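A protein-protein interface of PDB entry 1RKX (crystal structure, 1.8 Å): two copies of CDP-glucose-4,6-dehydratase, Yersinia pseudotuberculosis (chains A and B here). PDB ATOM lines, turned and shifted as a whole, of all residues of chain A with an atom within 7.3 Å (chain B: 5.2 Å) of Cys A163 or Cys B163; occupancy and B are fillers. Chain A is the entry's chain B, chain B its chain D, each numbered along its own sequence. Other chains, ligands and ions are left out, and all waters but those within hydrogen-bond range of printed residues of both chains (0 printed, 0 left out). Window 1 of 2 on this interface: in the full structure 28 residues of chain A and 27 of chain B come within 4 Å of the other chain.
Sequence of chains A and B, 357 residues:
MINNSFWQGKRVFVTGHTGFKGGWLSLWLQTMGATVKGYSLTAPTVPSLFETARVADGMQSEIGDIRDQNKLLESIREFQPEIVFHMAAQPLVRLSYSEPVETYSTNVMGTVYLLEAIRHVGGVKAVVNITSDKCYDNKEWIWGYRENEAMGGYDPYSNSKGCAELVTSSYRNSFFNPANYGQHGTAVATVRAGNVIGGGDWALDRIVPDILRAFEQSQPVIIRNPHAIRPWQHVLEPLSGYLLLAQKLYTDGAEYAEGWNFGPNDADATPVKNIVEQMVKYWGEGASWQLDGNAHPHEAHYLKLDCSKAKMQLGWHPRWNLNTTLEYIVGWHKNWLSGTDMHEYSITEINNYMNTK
O of Leu B166 is in hydrogen-bond range of ND2 of Asn A159, at 2.9 Å. O of Cys A163 sits at hydrogen-bond distance from SG of Cys B163, 3.7 Å away. OD1 of Asn A159 is in hydrogen-bond range of N of Val B167, 3.3 Å away. The backbone carbonyl oxygen (O) of Leu A166 sits at hydrogen-bond distance from the side-chain amide nitrogen (ND2) of Asn B159, at 3.0 Å. N of Val A167 lies within hydrogen-bond range of OD1 of Asn B159 (3.3 Å).
OD1 of Asn B159 is in hydrogen-bond range of OH of Tyr B104, 2.7 Å away. The backbone carbonyl oxygen of Asn A159 sits at hydrogen-bond distance from the side-chain sulfur of Cys A163 (3.5 Å). The backbone carbonyl oxygen (O) of Gly A153 lies within hydrogen-bond range of the side-chain amide nitrogen (ND2) of Asn A159, at 3.1 Å. The backbone carbonyl oxygen of Asn B159 sits at hydrogen-bond distance from the side-chain sulfur of Cys B163. OH of Tyr A104 sits at hydrogen-bond distance from OD1 of Asn A159 (2.7 Å). N of Gly A152 lies within hydrogen-bond range of O of Cys A135 (2.8 Å).
Among the printed residues, pairs that only touch across the chains: Tyr A104 with Val B167 (3.5 Å), Val A167 with Tyr B104 (3.6 Å), Gly A162 with Leu B166 (3.7 Å), Cys A163 with Leu B166 (3.7 Å), Leu A166 with Gly B162 (3.7 Å), Leu A166 with Cys B163 (3.7 Å), Gly A152 with Leu B166 (3.9 Å), Leu A166 with Gly B152 (3.9 Å) and Val A112 with Tyr B104 (3.9 Å).
Thr A111 touches none of the printed residues of chain B. Of the printed residues of chain B, Gly A152 touches Leu B166. Of the printed residues of chain B, Cys A163 touches Cys B163 (3.7 Å) and Leu B166 (3.7 Å). Printed residues of chain A within 4 Å of Tyr B104: Val A112 (3.9 Å) and Val A167 (3.6 Å). Gly B162 touches just one residue of chain A: Leu A166 (3.7 Å). Cys B163 touches just these residues of chain A: Cys A163 and Leu A166. Of the printed residues of chain A, Leu B166 touches Gly A152, Asn A159, Gly A162 and Cys A163. The nearest residue of chain B that does not touch Cys A163 is Val B167 (4.3 Å). The nearest residue of chain A that does not touch Cys B163 is Val A167 (4.3 Å). The nearest printed residue of chain A that does not touch Val B167 is Cys A163 (4.3 Å).
Of the 13 printed residues of chain B, 7 touch a printed residue of chain A. Hydrophobic or aromatic side chains of chain B within 4 Å of the printed part of chain A: Tyr B104, Leu B166 and Val B167. Hydrophobic or aromatic side chains of chain A within 4 Å of the printed part of chain B: Tyr A104, Val A112, Leu A166 and Val A167. Along chain A the printed residues that touch a printed residue of chain B span positions 104 to 167. Among the printed residues, no Asp or Glu carboxylate lies within 4 Å of a Lys or Arg side-chain nitrogen of the other chain.
Tyr A104 touches Val B167, and with the chains exchanged Val A167 touches Tyr B104. Gly A152 touches Leu B166, and with the chains exchanged Leu A166 touches Gly B152. Asn A159 touches Leu B166, and with the chains exchanged Leu A166 touches Asn B159. Gly A162 touches Leu B166, and with the chains exchanged Leu A166 touches Gly B162.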
ATOM      1  N   TYR A 104     -19.456  -2.936 -33.934  1.00  0.00           N
ATOM      2  CA  TYR A 104     -18.652  -3.715 -32.988  1.00  0.00           C
ATOM      3  C   TYR A 104     -17.179  -3.318 -33.018  1.00  0.00           C
ATOM      4  O   TYR A 104     -16.542  -3.215 -31.973  1.00  0.00           O
ATOM      5  CB  TYR A 104     -18.777  -5.215 -33.263  1.00  0.00           C
ATOM      6  CG  TYR A 104     -20.015  -5.838 -32.663  1.00  0.00           C
ATOM      7  CD1 TYR A 104     -21.084  -6.238 -33.469  1.00  0.00           C
ATOM      8  CD2 TYR A 104     -20.119  -6.033 -31.285  1.00  0.00           C
ATOM      9  CE1 TYR A 104     -22.224  -6.819 -32.915  1.00  0.00           C
ATOM     10  CE2 TYR A 104     -21.253  -6.605 -30.717  1.00  0.00           C
ATOM     11  CZ  TYR A 104     -22.302  -6.995 -31.535  1.00  0.00           C
ATOM     12  OH  TYR A 104     -23.433  -7.544 -30.975  1.00  0.00           O
ATOM     13  N   ASN A 107     -17.139   0.288 -31.280  1.00  0.00           N
ATOM     14  CA  ASN A 107     -17.474   0.301 -29.862  1.00  0.00           C
ATOM     15  C   ASN A 107     -16.719  -0.683 -28.984  1.00  0.00           C
ATOM     16  O   ASN A 107     -16.406  -0.362 -27.836  1.00  0.00           O
ATOM     17  CB  ASN A 107     -18.984   0.128 -29.687  1.00  0.00           C
ATOM     18  CG  ASN A 107     -19.773   1.231 -30.385  1.00  0.00           C
ATOM     19  OD1 ASN A 107     -19.194   2.188 -30.916  1.00  0.00           O
ATOM     20  ND2 ASN A 107     -21.091   1.109 -30.386  1.00  0.00           N
ATOM     21  N   VAL A 108     -16.420  -1.867 -29.512  1.00  0.00           N
ATOM     22  CA  VAL A 108     -15.685  -2.854 -28.732  1.00  0.00           C
ATOM     23  C   VAL A 108     -14.175  -2.727 -28.939  1.00  0.00           C
ATOM     24  O   VAL A 108     -13.453  -2.433 -27.991  1.00  0.00           O
ATOM     25  CB  VAL A 108     -16.136  -4.291 -29.068  1.00  0.00           C
ATOM     26  CG1 VAL A 108     -15.363  -5.292 -28.210  1.00  0.00           C
ATOM     27  CG2 VAL A 108     -17.635  -4.430 -28.825  1.00  0.00           C
ATOM     28  N   THR A 111     -12.683   0.575 -27.817  1.00  0.00           N
ATOM     29  CA  THR A 111     -12.508   0.643 -26.372  1.00  0.00           C
ATOM     30  C   THR A 111     -11.266  -0.165 -25.985  1.00  0.00           C
ATOM     31  O   THR A 111     -10.467   0.269 -25.147  1.00  0.00           O
ATOM     32  CB  THR A 111     -13.761   0.100 -25.644  1.00  0.00           C
ATOM     33  OG1 THR A 111     -14.885   0.923 -25.971  1.00  0.00           O
ATOM     34  CG2 THR A 111     -13.565   0.106 -24.144  1.00  0.00           C
ATOM     35  N   VAL A 112     -11.090  -1.334 -26.601  1.00  0.00           N
ATOM     36  CA  VAL A 112      -9.908  -2.155 -26.326  1.00  0.00           C
ATOM     37  C   VAL A 112      -8.621  -1.381 -26.663  1.00  0.00           C
ATOM     38  O   VAL A 112      -7.681  -1.348 -25.868  1.00  0.00           O
ATOM     39  CB  VAL A 112      -9.926  -3.469 -27.141  1.00  0.00           C
ATOM     40  CG1 VAL A 112      -8.565  -4.166 -27.046  1.00  0.00           C
ATOM     41  CG2 VAL A 112     -11.027  -4.389 -26.609  1.00  0.00           C
ATOM     42  N   THR A 131     -20.317   4.288 -21.847  1.00  0.00           N
ATOM     43  CA  THR A 131     -20.894   3.164 -22.560  1.00  0.00           C
ATOM     44  C   THR A 131     -22.305   3.581 -22.971  1.00  0.00           C
ATOM     45  O   THR A 131     -22.465   4.349 -23.930  1.00  0.00           O
ATOM     46  CB  THR A 131     -20.885   1.880 -21.691  1.00  0.00           C
ATOM     47  OG1 THR A 131     -21.590   2.102 -20.464  1.00  0.00           O
ATOM     48  CG2 THR A 131     -19.440   1.485 -21.374  1.00  0.00           C
ATOM     49  N   CYS A 135     -26.570  -0.764 -22.168  1.00  0.00           N
ATOM     50  CA  CYS A 135     -25.656  -1.890 -21.989  1.00  0.00           C
ATOM     51  C   CYS A 135     -26.277  -3.043 -21.196  1.00  0.00           C
ATOM     52  O   CYS A 135     -25.754  -4.157 -21.208  1.00  0.00           O
ATOM     53  CB  CYS A 135     -24.380  -1.436 -21.269  1.00  0.00           C
ATOM     54  SG  CYS A 135     -24.681  -0.894 -19.557  1.00  0.00           S
ATOM     55  N   MET A 151     -25.167  -7.608 -18.212  1.00  0.00           N
ATOM     56  CA  MET A 151     -24.899  -6.845 -19.422  1.00  0.00           C
ATOM     57  C   MET A 151     -25.484  -7.617 -20.606  1.00  0.00           C
ATOM     58  O   MET A 151     -25.648  -8.836 -20.552  1.00  0.00           O
ATOM     59  CB  MET A 151     -23.391  -6.669 -19.619  1.00  0.00           C
ATOM     60  CG  MET A 151     -22.695  -5.861 -18.529  1.00  0.00           C
ATOM     61  SD  MET A 151     -23.171  -4.116 -18.558  1.00  0.00           S
ATOM     62  CE  MET A 151     -24.446  -4.102 -17.300  1.00  0.00           C
ATOM     63  N   GLY A 152     -25.802  -6.901 -21.675  1.00  0.00           N
ATOM     64  CA  GLY A 152     -26.366  -7.552 -22.841  1.00  0.00           C
ATOM     65  C   GLY A 152     -26.693  -6.550 -23.927  1.00  0.00           C
ATOM     66  O   GLY A 152     -25.890  -5.668 -24.237  1.00  0.00           O
ATOM     67  N   GLY A 153     -27.879  -6.679 -24.503  1.00  0.00           N
ATOM     68  CA  GLY A 153     -28.283  -5.777 -25.561  1.00  0.00           C
ATOM     69  C   GLY A 153     -28.864  -6.529 -26.744  1.00  0.00           C
ATOM     70  O   GLY A 153     -28.271  -7.483 -27.247  1.00  0.00           O
ATOM     71  N   PRO A 156     -27.212  -4.599 -32.298  1.00  0.00           N
ATOM     72  CA  PRO A 156     -25.746  -4.519 -32.299  1.00  0.00           C
ATOM     73  C   PRO A 156     -25.175  -3.344 -31.502  1.00  0.00           C
ATOM     74  O   PRO A 156     -24.139  -3.481 -30.848  1.00  0.00           O
ATOM     75  CB  PRO A 156     -25.412  -4.438 -33.785  1.00  0.00           C
ATOM     76  CG  PRO A 156     -26.500  -5.288 -34.404  1.00  0.00           C
ATOM     77  CD  PRO A 156     -27.724  -4.798 -33.667  1.00  0.00           C
ATOM     78  N   TYR A 157     -25.834  -2.190 -31.560  1.00  0.00           N
ATOM     79  CA  TYR A 157     -25.353  -1.030 -30.811  1.00  0.00           C
ATOM     80  C   TYR A 157     -25.421  -1.296 -29.307  1.00  0.00           C
ATOM     81  O   TYR A 157     -24.414  -1.192 -28.597  1.00  0.00           O
ATOM     82  CB  TYR A 157     -26.174   0.218 -31.134  1.00  0.00           C
ATOM     83  CG  TYR A 157     -26.080   1.272 -30.053  1.00  0.00           C
ATOM     84  CD1 TYR A 157     -24.932   2.046 -29.904  1.00  0.00           C
ATOM     85  CD2 TYR A 157     -27.115   1.442 -29.133  1.00  0.00           C
ATOM     86  CE1 TYR A 157     -24.816   2.969 -28.859  1.00  0.00           C
ATOM     87  CE2 TYR A 157     -27.010   2.357 -28.084  1.00  0.00           C
ATOM     88  CZ  TYR A 157     -25.861   3.113 -27.955  1.00  0.00           C
ATOM     89  OH  TYR A 157     -25.756   4.005 -26.914  1.00  0.00           O
ATOM     90  N   SER A 158     -26.615  -1.623 -28.828  1.00  0.00           N
ATOM     91  CA  SER A 158     -26.818  -1.909 -27.410  1.00  0.00           C
ATOM     92  C   SER A 158     -25.871  -3.012 -26.957  1.00  0.00           C
ATOM     93  O   SER A 158     -25.213  -2.888 -25.925  1.00  0.00           O
ATOM     94  CB  SER A 158     -28.267  -2.343 -27.156  1.00  0.00           C
ATOM     95  OG  SER A 158     -29.171  -1.300 -27.499  1.00  0.00           O
ATOM     96  N   ASN A 159     -25.804  -4.081 -27.741  1.00  0.00           N
ATOM     97  CA  ASN A 159     -24.954  -5.215 -27.407  1.00  0.00           C
ATOM     98  C   ASN A 159     -23.468  -4.860 -27.404  1.00  0.00           C
ATOM     99  O   ASN A 159     -22.707  -5.363 -26.568  1.00  0.00           O
ATOM    100  CB  ASN A 159     -25.223  -6.367 -28.381  1.00  0.00           C
ATOM    101  CG  ASN A 159     -24.629  -7.663 -27.910  1.00  0.00           C
ATOM    102  OD1 ASN A 159     -23.523  -8.019 -28.296  1.00  0.00           O
ATOM    103  ND2 ASN A 159     -25.355  -8.367 -27.046  1.00  0.00           N
ATOM    104  N   SER A 160     -23.050  -3.995 -28.325  1.00  0.00           N
ATOM    105  CA  SER A 160     -21.644  -3.598 -28.390  1.00  0.00           C
ATOM    106  C   SER A 160     -21.275  -2.816 -27.137  1.00  0.00           C
ATOM    107  O   SER A 160     -20.134  -2.850 -26.696  1.00  0.00           O
ATOM    108  CB  SER A 160     -21.359  -2.753 -29.640  1.00  0.00           C
ATOM    109  OG  SER A 160     -21.903  -1.446 -29.552  1.00  0.00           O
ATOM    110  N   LYS A 161     -22.249  -2.113 -26.563  1.00  0.00           N
ATOM    111  CA  LYS A 161     -22.010  -1.347 -25.346  1.00  0.00           C
ATOM    112  C   LYS A 161     -21.926  -2.306 -24.161  1.00  0.00           C
ATOM    113  O   LYS A 161     -21.161  -2.073 -23.219  1.00  0.00           O
ATOM    114  CB  LYS A 161     -23.114  -0.314 -25.140  1.00  0.00           C
ATOM    115  CG  LYS A 161     -23.042   0.858 -26.133  1.00  0.00           C
ATOM    116  CD  LYS A 161     -21.786   1.690 -25.900  1.00  0.00           C
ATOM    117  CE  LYS A 161     -21.779   2.965 -26.729  1.00  0.00           C
ATOM    118  NZ  LYS A 161     -20.695   3.907 -26.302  1.00  0.00           N
ATOM    119  N   GLY A 162     -22.715  -3.380 -24.212  1.00  0.00           N
ATOM    120  CA  GLY A 162     -22.654  -4.392 -23.167  1.00  0.00           C
ATOM    121  C   GLY A 162     -21.258  -5.012 -23.239  1.00  0.00           C
ATOM    122  O   GLY A 162     -20.619  -5.271 -22.211  1.00  0.00           O
ATOM    123  N   CYS A 163     -20.767  -5.233 -24.459  1.00  0.00           N
ATOM    124  CA  CYS A 163     -19.427  -5.792 -24.630  1.00  0.00           C
ATOM    125  C   CYS A 163     -18.360  -4.823 -24.113  1.00  0.00           C
ATOM    126  O   CYS A 163     -17.386  -5.248 -23.498  1.00  0.00           O
ATOM    127  CB  CYS A 163     -19.147  -6.104 -26.101  1.00  0.00           C
ATOM    128  SG  CYS A 163     -19.993  -7.582 -26.711  1.00  0.00           S
ATOM    129  N   ALA A 164     -18.543  -3.533 -24.383  1.00  0.00           N
ATOM    130  CA  ALA A 164     -17.592  -2.510 -23.934  1.00  0.00           C
ATOM    131  C   ALA A 164     -17.479  -2.534 -22.411  1.00  0.00           C
ATOM    132  O   ALA A 164     -16.400  -2.313 -21.850  1.00  0.00           O
ATOM    133  CB  ALA A 164     -18.037  -1.126 -24.414  1.00  0.00           C
ATOM    134  N   GLU A 165     -18.598  -2.806 -21.743  1.00  0.00           N
ATOM    135  CA  GLU A 165     -18.610  -2.895 -20.289  1.00  0.00           C
ATOM    136  C   GLU A 165     -17.753  -4.088 -19.874  1.00  0.00           C
ATOM    137  O   GLU A 165     -16.903  -3.970 -18.991  1.00  0.00           O
ATOM    138  CB  GLU A 165     -20.045  -3.067 -19.772  1.00  0.00           C
ATOM    139  CG  GLU A 165     -20.857  -1.766 -19.700  1.00  0.00           C
ATOM    140  CD  GLU A 165     -20.422  -0.845 -18.560  1.00  0.00           C
ATOM    141  OE1 GLU A 165     -19.673  -1.292 -17.657  1.00  0.00           O
ATOM    142  OE2 GLU A 165     -20.845   0.328 -18.549  1.00  0.00           O
ATOM    143  N   LEU A 166     -17.977  -5.241 -20.509  1.00  0.00           N
ATOM    144  CA  LEU A 166     -17.187  -6.428 -20.192  1.00  0.00           C
ATOM    145  C   LEU A 166     -15.692  -6.154 -20.409  1.00  0.00           C
ATOM    146  O   LEU A 166     -14.871  -6.454 -19.545  1.00  0.00           O
ATOM    147  CB  LEU A 166     -17.630  -7.621 -21.052  1.00  0.00           C
ATOM    148  CG  LEU A 166     -18.604  -8.597 -20.377  1.00  0.00           C
ATOM    149  CD1 LEU A 166     -19.912  -7.893 -20.056  1.00  0.00           C
ATOM    150  CD2 LEU A 166     -18.846  -9.799 -21.290  1.00  0.00           C
ATOM    151  N   VAL A 167     -15.350  -5.567 -21.556  1.00  0.00           N
ATOM    152  CA  VAL A 167     -13.958  -5.257 -21.876  1.00  0.00           C
ATOM    153  C   VAL A 167     -13.315  -4.407 -20.784  1.00  0.00           C
ATOM    154  O   VAL A 167     -12.211  -4.707 -20.329  1.00  0.00           O
ATOM    155  CB  VAL A 167     -13.843  -4.488 -23.217  1.00  0.00           C
ATOM    156  CG1 VAL A 167     -12.443  -3.889 -23.363  1.00  0.00           C
ATOM    157  CG2 VAL A 167     -14.121  -5.434 -24.386  1.00  0.00           C
ATOM    158  N   THR A 168     -14.007  -3.349 -20.373  1.00  0.00           N
ATOM    159  CA  THR A 168     -13.483  -2.452 -19.345  1.00  0.00           C
ATOM    160  C   THR A 168     -13.286  -3.199 -18.031  1.00  0.00           C
ATOM    161  O   THR A 168     -12.281  -3.014 -17.351  1.00  0.00           O
ATOM    162  CB  THR A 168     -14.420  -1.241 -19.129  1.00  0.00           C
ATOM    163  OG1 THR A 168     -14.651  -0.590 -20.385  1.00  0.00           O
ATOM    164  CG2 THR A 168     -13.767  -0.234 -18.172  1.00  0.00           C
ATOM    165  N   SER A 169     -14.246  -4.051 -17.680  1.00  0.00           N
ATOM    166  CA  SER A 169     -14.155  -4.843 -16.462  1.00  0.00           C
ATOM    167  C   SER A 169     -12.913  -5.742 -16.470  1.00  0.00           C
ATOM    168  O   SER A 169     -12.187  -5.814 -15.479  1.00  0.00           O
ATOM    169  CB  SER A 169     -15.408  -5.702 -16.295  1.00  0.00           C
ATOM    170  OG  SER A 169     -15.325  -6.510 -15.134  1.00  0.00           O
ATOM    171  N   TYR B 104      -9.093 -10.346 -28.041  1.00  0.00           N
ATOM    172  CA  TYR B 104     -10.397  -9.739 -28.355  1.00  0.00           C
ATOM    173  C   TYR B 104     -10.686  -9.684 -29.853  1.00  0.00           C
ATOM    174  O   TYR B 104     -11.799  -9.988 -30.287  1.00  0.00           O
ATOM    175  CB  TYR B 104     -10.508  -8.328 -27.765  1.00  0.00           C
ATOM    176  CG  TYR B 104     -10.874  -8.309 -26.295  1.00  0.00           C
ATOM    177  CD1 TYR B 104      -9.934  -7.968 -25.324  1.00  0.00           C
ATOM    178  CD2 TYR B 104     -12.169  -8.628 -25.878  1.00  0.00           C
ATOM    179  CE1 TYR B 104     -10.274  -7.943 -23.965  1.00  0.00           C
ATOM    180  CE2 TYR B 104     -12.519  -8.611 -24.528  1.00  0.00           C
ATOM    181  CZ  TYR B 104     -11.568  -8.268 -23.577  1.00  0.00           C
ATOM    182  OH  TYR B 104     -11.920  -8.259 -22.251  1.00  0.00           O
ATOM    183  N   VAL B 108     -13.760 -11.962 -30.405  1.00  0.00           N
ATOM    184  CA  VAL B 108     -14.944 -11.138 -30.594  1.00  0.00           C
ATOM    185  C   VAL B 108     -15.155 -10.764 -32.066  1.00  0.00           C
ATOM    186  O   VAL B 108     -16.163 -11.147 -32.649  1.00  0.00           O
ATOM    187  CB  VAL B 108     -14.886  -9.855 -29.735  1.00  0.00           C
ATOM    188  CG1 VAL B 108     -16.161  -9.047 -29.930  1.00  0.00           C
ATOM    189  CG2 VAL B 108     -14.716 -10.223 -28.258  1.00  0.00           C
ATOM    190  N   GLY B 152     -19.614 -12.732 -18.582  1.00  0.00           N
ATOM    191  CA  GLY B 152     -18.556 -11.896 -18.054  1.00  0.00           C
ATOM    192  C   GLY B 152     -17.197 -12.505 -18.311  1.00  0.00           C
ATOM    193  O   GLY B 152     -16.918 -12.961 -19.417  1.00  0.00           O
ATOM    194  N   ASN B 159     -13.280 -13.175 -20.697  1.00  0.00           N
ATOM    195  CA  ASN B 159     -14.129 -12.034 -21.019  1.00  0.00           C
ATOM    196  C   ASN B 159     -14.466 -11.943 -22.511  1.00  0.00           C
ATOM    197  O   ASN B 159     -15.591 -11.576 -22.876  1.00  0.00           O
ATOM    198  CB  ASN B 159     -13.458 -10.741 -20.543  1.00  0.00           C
ATOM    199  CG  ASN B 159     -14.411  -9.565 -20.527  1.00  0.00           C
ATOM    200  OD1 ASN B 159     -14.472  -8.788 -21.476  1.00  0.00           O
ATOM    201  ND2 ASN B 159     -15.169  -9.437 -19.442  1.00  0.00           N
ATOM    202  N   SER B 160     -13.507 -12.278 -23.373  1.00  0.00           N
ATOM    203  CA  SER B 160     -13.758 -12.226 -24.814  1.00  0.00           C
ATOM    204  C   SER B 160     -14.816 -13.258 -25.189  1.00  0.00           C
ATOM    205  O   SER B 160     -15.567 -13.062 -26.147  1.00  0.00           O
ATOM    206  CB  SER B 160     -12.472 -12.489 -25.612  1.00  0.00           C
ATOM    207  OG  SER B 160     -12.064 -13.846 -25.545  1.00  0.00           O
ATOM    208  N   LYS B 161     -14.879 -14.353 -24.433  1.00  0.00           N
ATOM    209  CA  LYS B 161     -15.865 -15.403 -24.697  1.00  0.00           C
ATOM    210  C   LYS B 161     -17.235 -14.928 -24.215  1.00  0.00           C
ATOM    211  O   LYS B 161     -18.268 -15.245 -24.818  1.00  0.00           O
ATOM    212  CB  LYS B 161     -15.452 -16.712 -24.010  1.00  0.00           C
ATOM    213  CG  LYS B 161     -14.253 -17.404 -24.676  1.00  0.00           C
ATOM    214  CD  LYS B 161     -14.621 -17.900 -26.085  1.00  0.00           C
ATOM    215  CE  LYS B 161     -13.516 -18.748 -26.698  1.00  0.00           C
ATOM    216  NZ  LYS B 161     -13.994 -19.421 -27.938  1.00  0.00           N
ATOM    217  N   GLY B 162     -17.242 -14.160 -23.129  1.00  0.00           N
ATOM    218  CA  GLY B 162     -18.491 -13.600 -22.636  1.00  0.00           C
ATOM    219  C   GLY B 162     -18.989 -12.632 -23.706  1.00  0.00           C
ATOM    220  O   GLY B 162     -20.183 -12.571 -23.993  1.00  0.00           O
ATOM    221  N   CYS B 163     -18.070 -11.877 -24.311  1.00  0.00           N
ATOM    222  CA  CYS B 163     -18.433 -10.944 -25.382  1.00  0.00           C
ATOM    223  C   CYS B 163     -18.949 -11.698 -26.612  1.00  0.00           C
ATOM    224  O   CYS B 163     -19.897 -11.256 -27.265  1.00  0.00           O
ATOM    225  CB  CYS B 163     -17.238 -10.083 -25.789  1.00  0.00           C
ATOM    226  SG  CYS B 163     -16.850  -8.743 -24.600  1.00  0.00           S
ATOM    227  N   ALA B 164     -18.307 -12.819 -26.939  1.00  0.00           N
ATOM    228  CA  ALA B 164     -18.724 -13.626 -28.091  1.00  0.00           C
ATOM    229  C   ALA B 164     -20.165 -14.097 -27.906  1.00  0.00           C
ATOM    230  O   ALA B 164     -20.932 -14.190 -28.874  1.00  0.00           O
ATOM    231  CB  ALA B 164     -17.790 -14.822 -28.262  1.00  0.00           C
ATOM    232  N   GLU B 165     -20.533 -14.390 -26.661  1.00  0.00           N
ATOM    233  CA  GLU B 165     -21.893 -14.816 -26.353  1.00  0.00           C
ATOM    234  C   GLU B 165     -22.837 -13.645 -26.628  1.00  0.00           C
ATOM    235  O   GLU B 165     -23.877 -13.814 -27.271  1.00  0.00           O
ATOM    236  CB  GLU B 165     -22.009 -15.253 -24.882  1.00  0.00           C
ATOM    237  CG  GLU B 165     -21.498 -16.664 -24.578  1.00  0.00           C
ATOM    238  CD  GLU B 165     -22.439 -17.765 -25.088  1.00  0.00           C
ATOM    239  OE1 GLU B 165     -23.595 -17.460 -25.436  1.00  0.00           O
ATOM    240  OE2 GLU B 165     -22.031 -18.939 -25.116  1.00  0.00           O
ATOM    241  N   LEU B 166     -22.484 -12.456 -26.143  1.00  0.00           N
ATOM    242  CA  LEU B 166     -23.325 -11.280 -26.384  1.00  0.00           C
ATOM    243  C   LEU B 166     -23.484 -11.038 -27.891  1.00  0.00           C
ATOM    244  O   LEU B 166     -24.596 -10.825 -28.388  1.00  0.00           O
ATOM    245  CB  LEU B 166     -22.724 -10.035 -25.712  1.00  0.00           C
ATOM    246  CG  LEU B 166     -23.315  -9.663 -24.343  1.00  0.00           C
ATOM    247  CD1 LEU B 166     -23.024 -10.760 -23.327  1.00  0.00           C
ATOM    248  CD2 LEU B 166     -22.735  -8.335 -23.870  1.00  0.00           C
ATOM    249  N   VAL B 167     -22.371 -11.081 -28.618  1.00  0.00           N
ATOM    250  CA  VAL B 167     -22.398 -10.866 -30.067  1.00  0.00           C
ATOM    251  C   VAL B 167     -23.365 -11.830 -30.753  1.00  0.00           C
ATOM    252  O   VAL B 167     -24.186 -11.417 -31.566  1.00  0.00           O
ATOM    253  CB  VAL B 167     -20.999 -11.057 -30.691  1.00  0.00           C
ATOM    254  CG1 VAL B 167     -21.108 -11.164 -32.215  1.00  0.00           C
ATOM    255  CG2 VAL B 167     -20.104  -9.882 -30.323  1.00  0.00           C
ATOM    256  N   THR B 168     -23.256 -13.112 -30.422  1.00  0.00           N
ATOM    257  CA  THR B 168     -24.116 -14.124 -31.023  1.00  0.00           C
ATOM    258  C   THR B 168     -25.574 -13.850 -30.694  1.00  0.00           C
ATOM    259  O   THR B 168     -26.442 -13.986 -31.553  1.00  0.00           O
ATOM    260  CB  THR B 168     -23.742 -15.541 -30.552  1.00  0.00           C
ATOM    261  OG1 THR B 168     -22.344 -15.766 -30.774  1.00  0.00           O
ATOM    262  CG2 THR B 168     -24.534 -16.592 -31.343  1.00  0.00           C
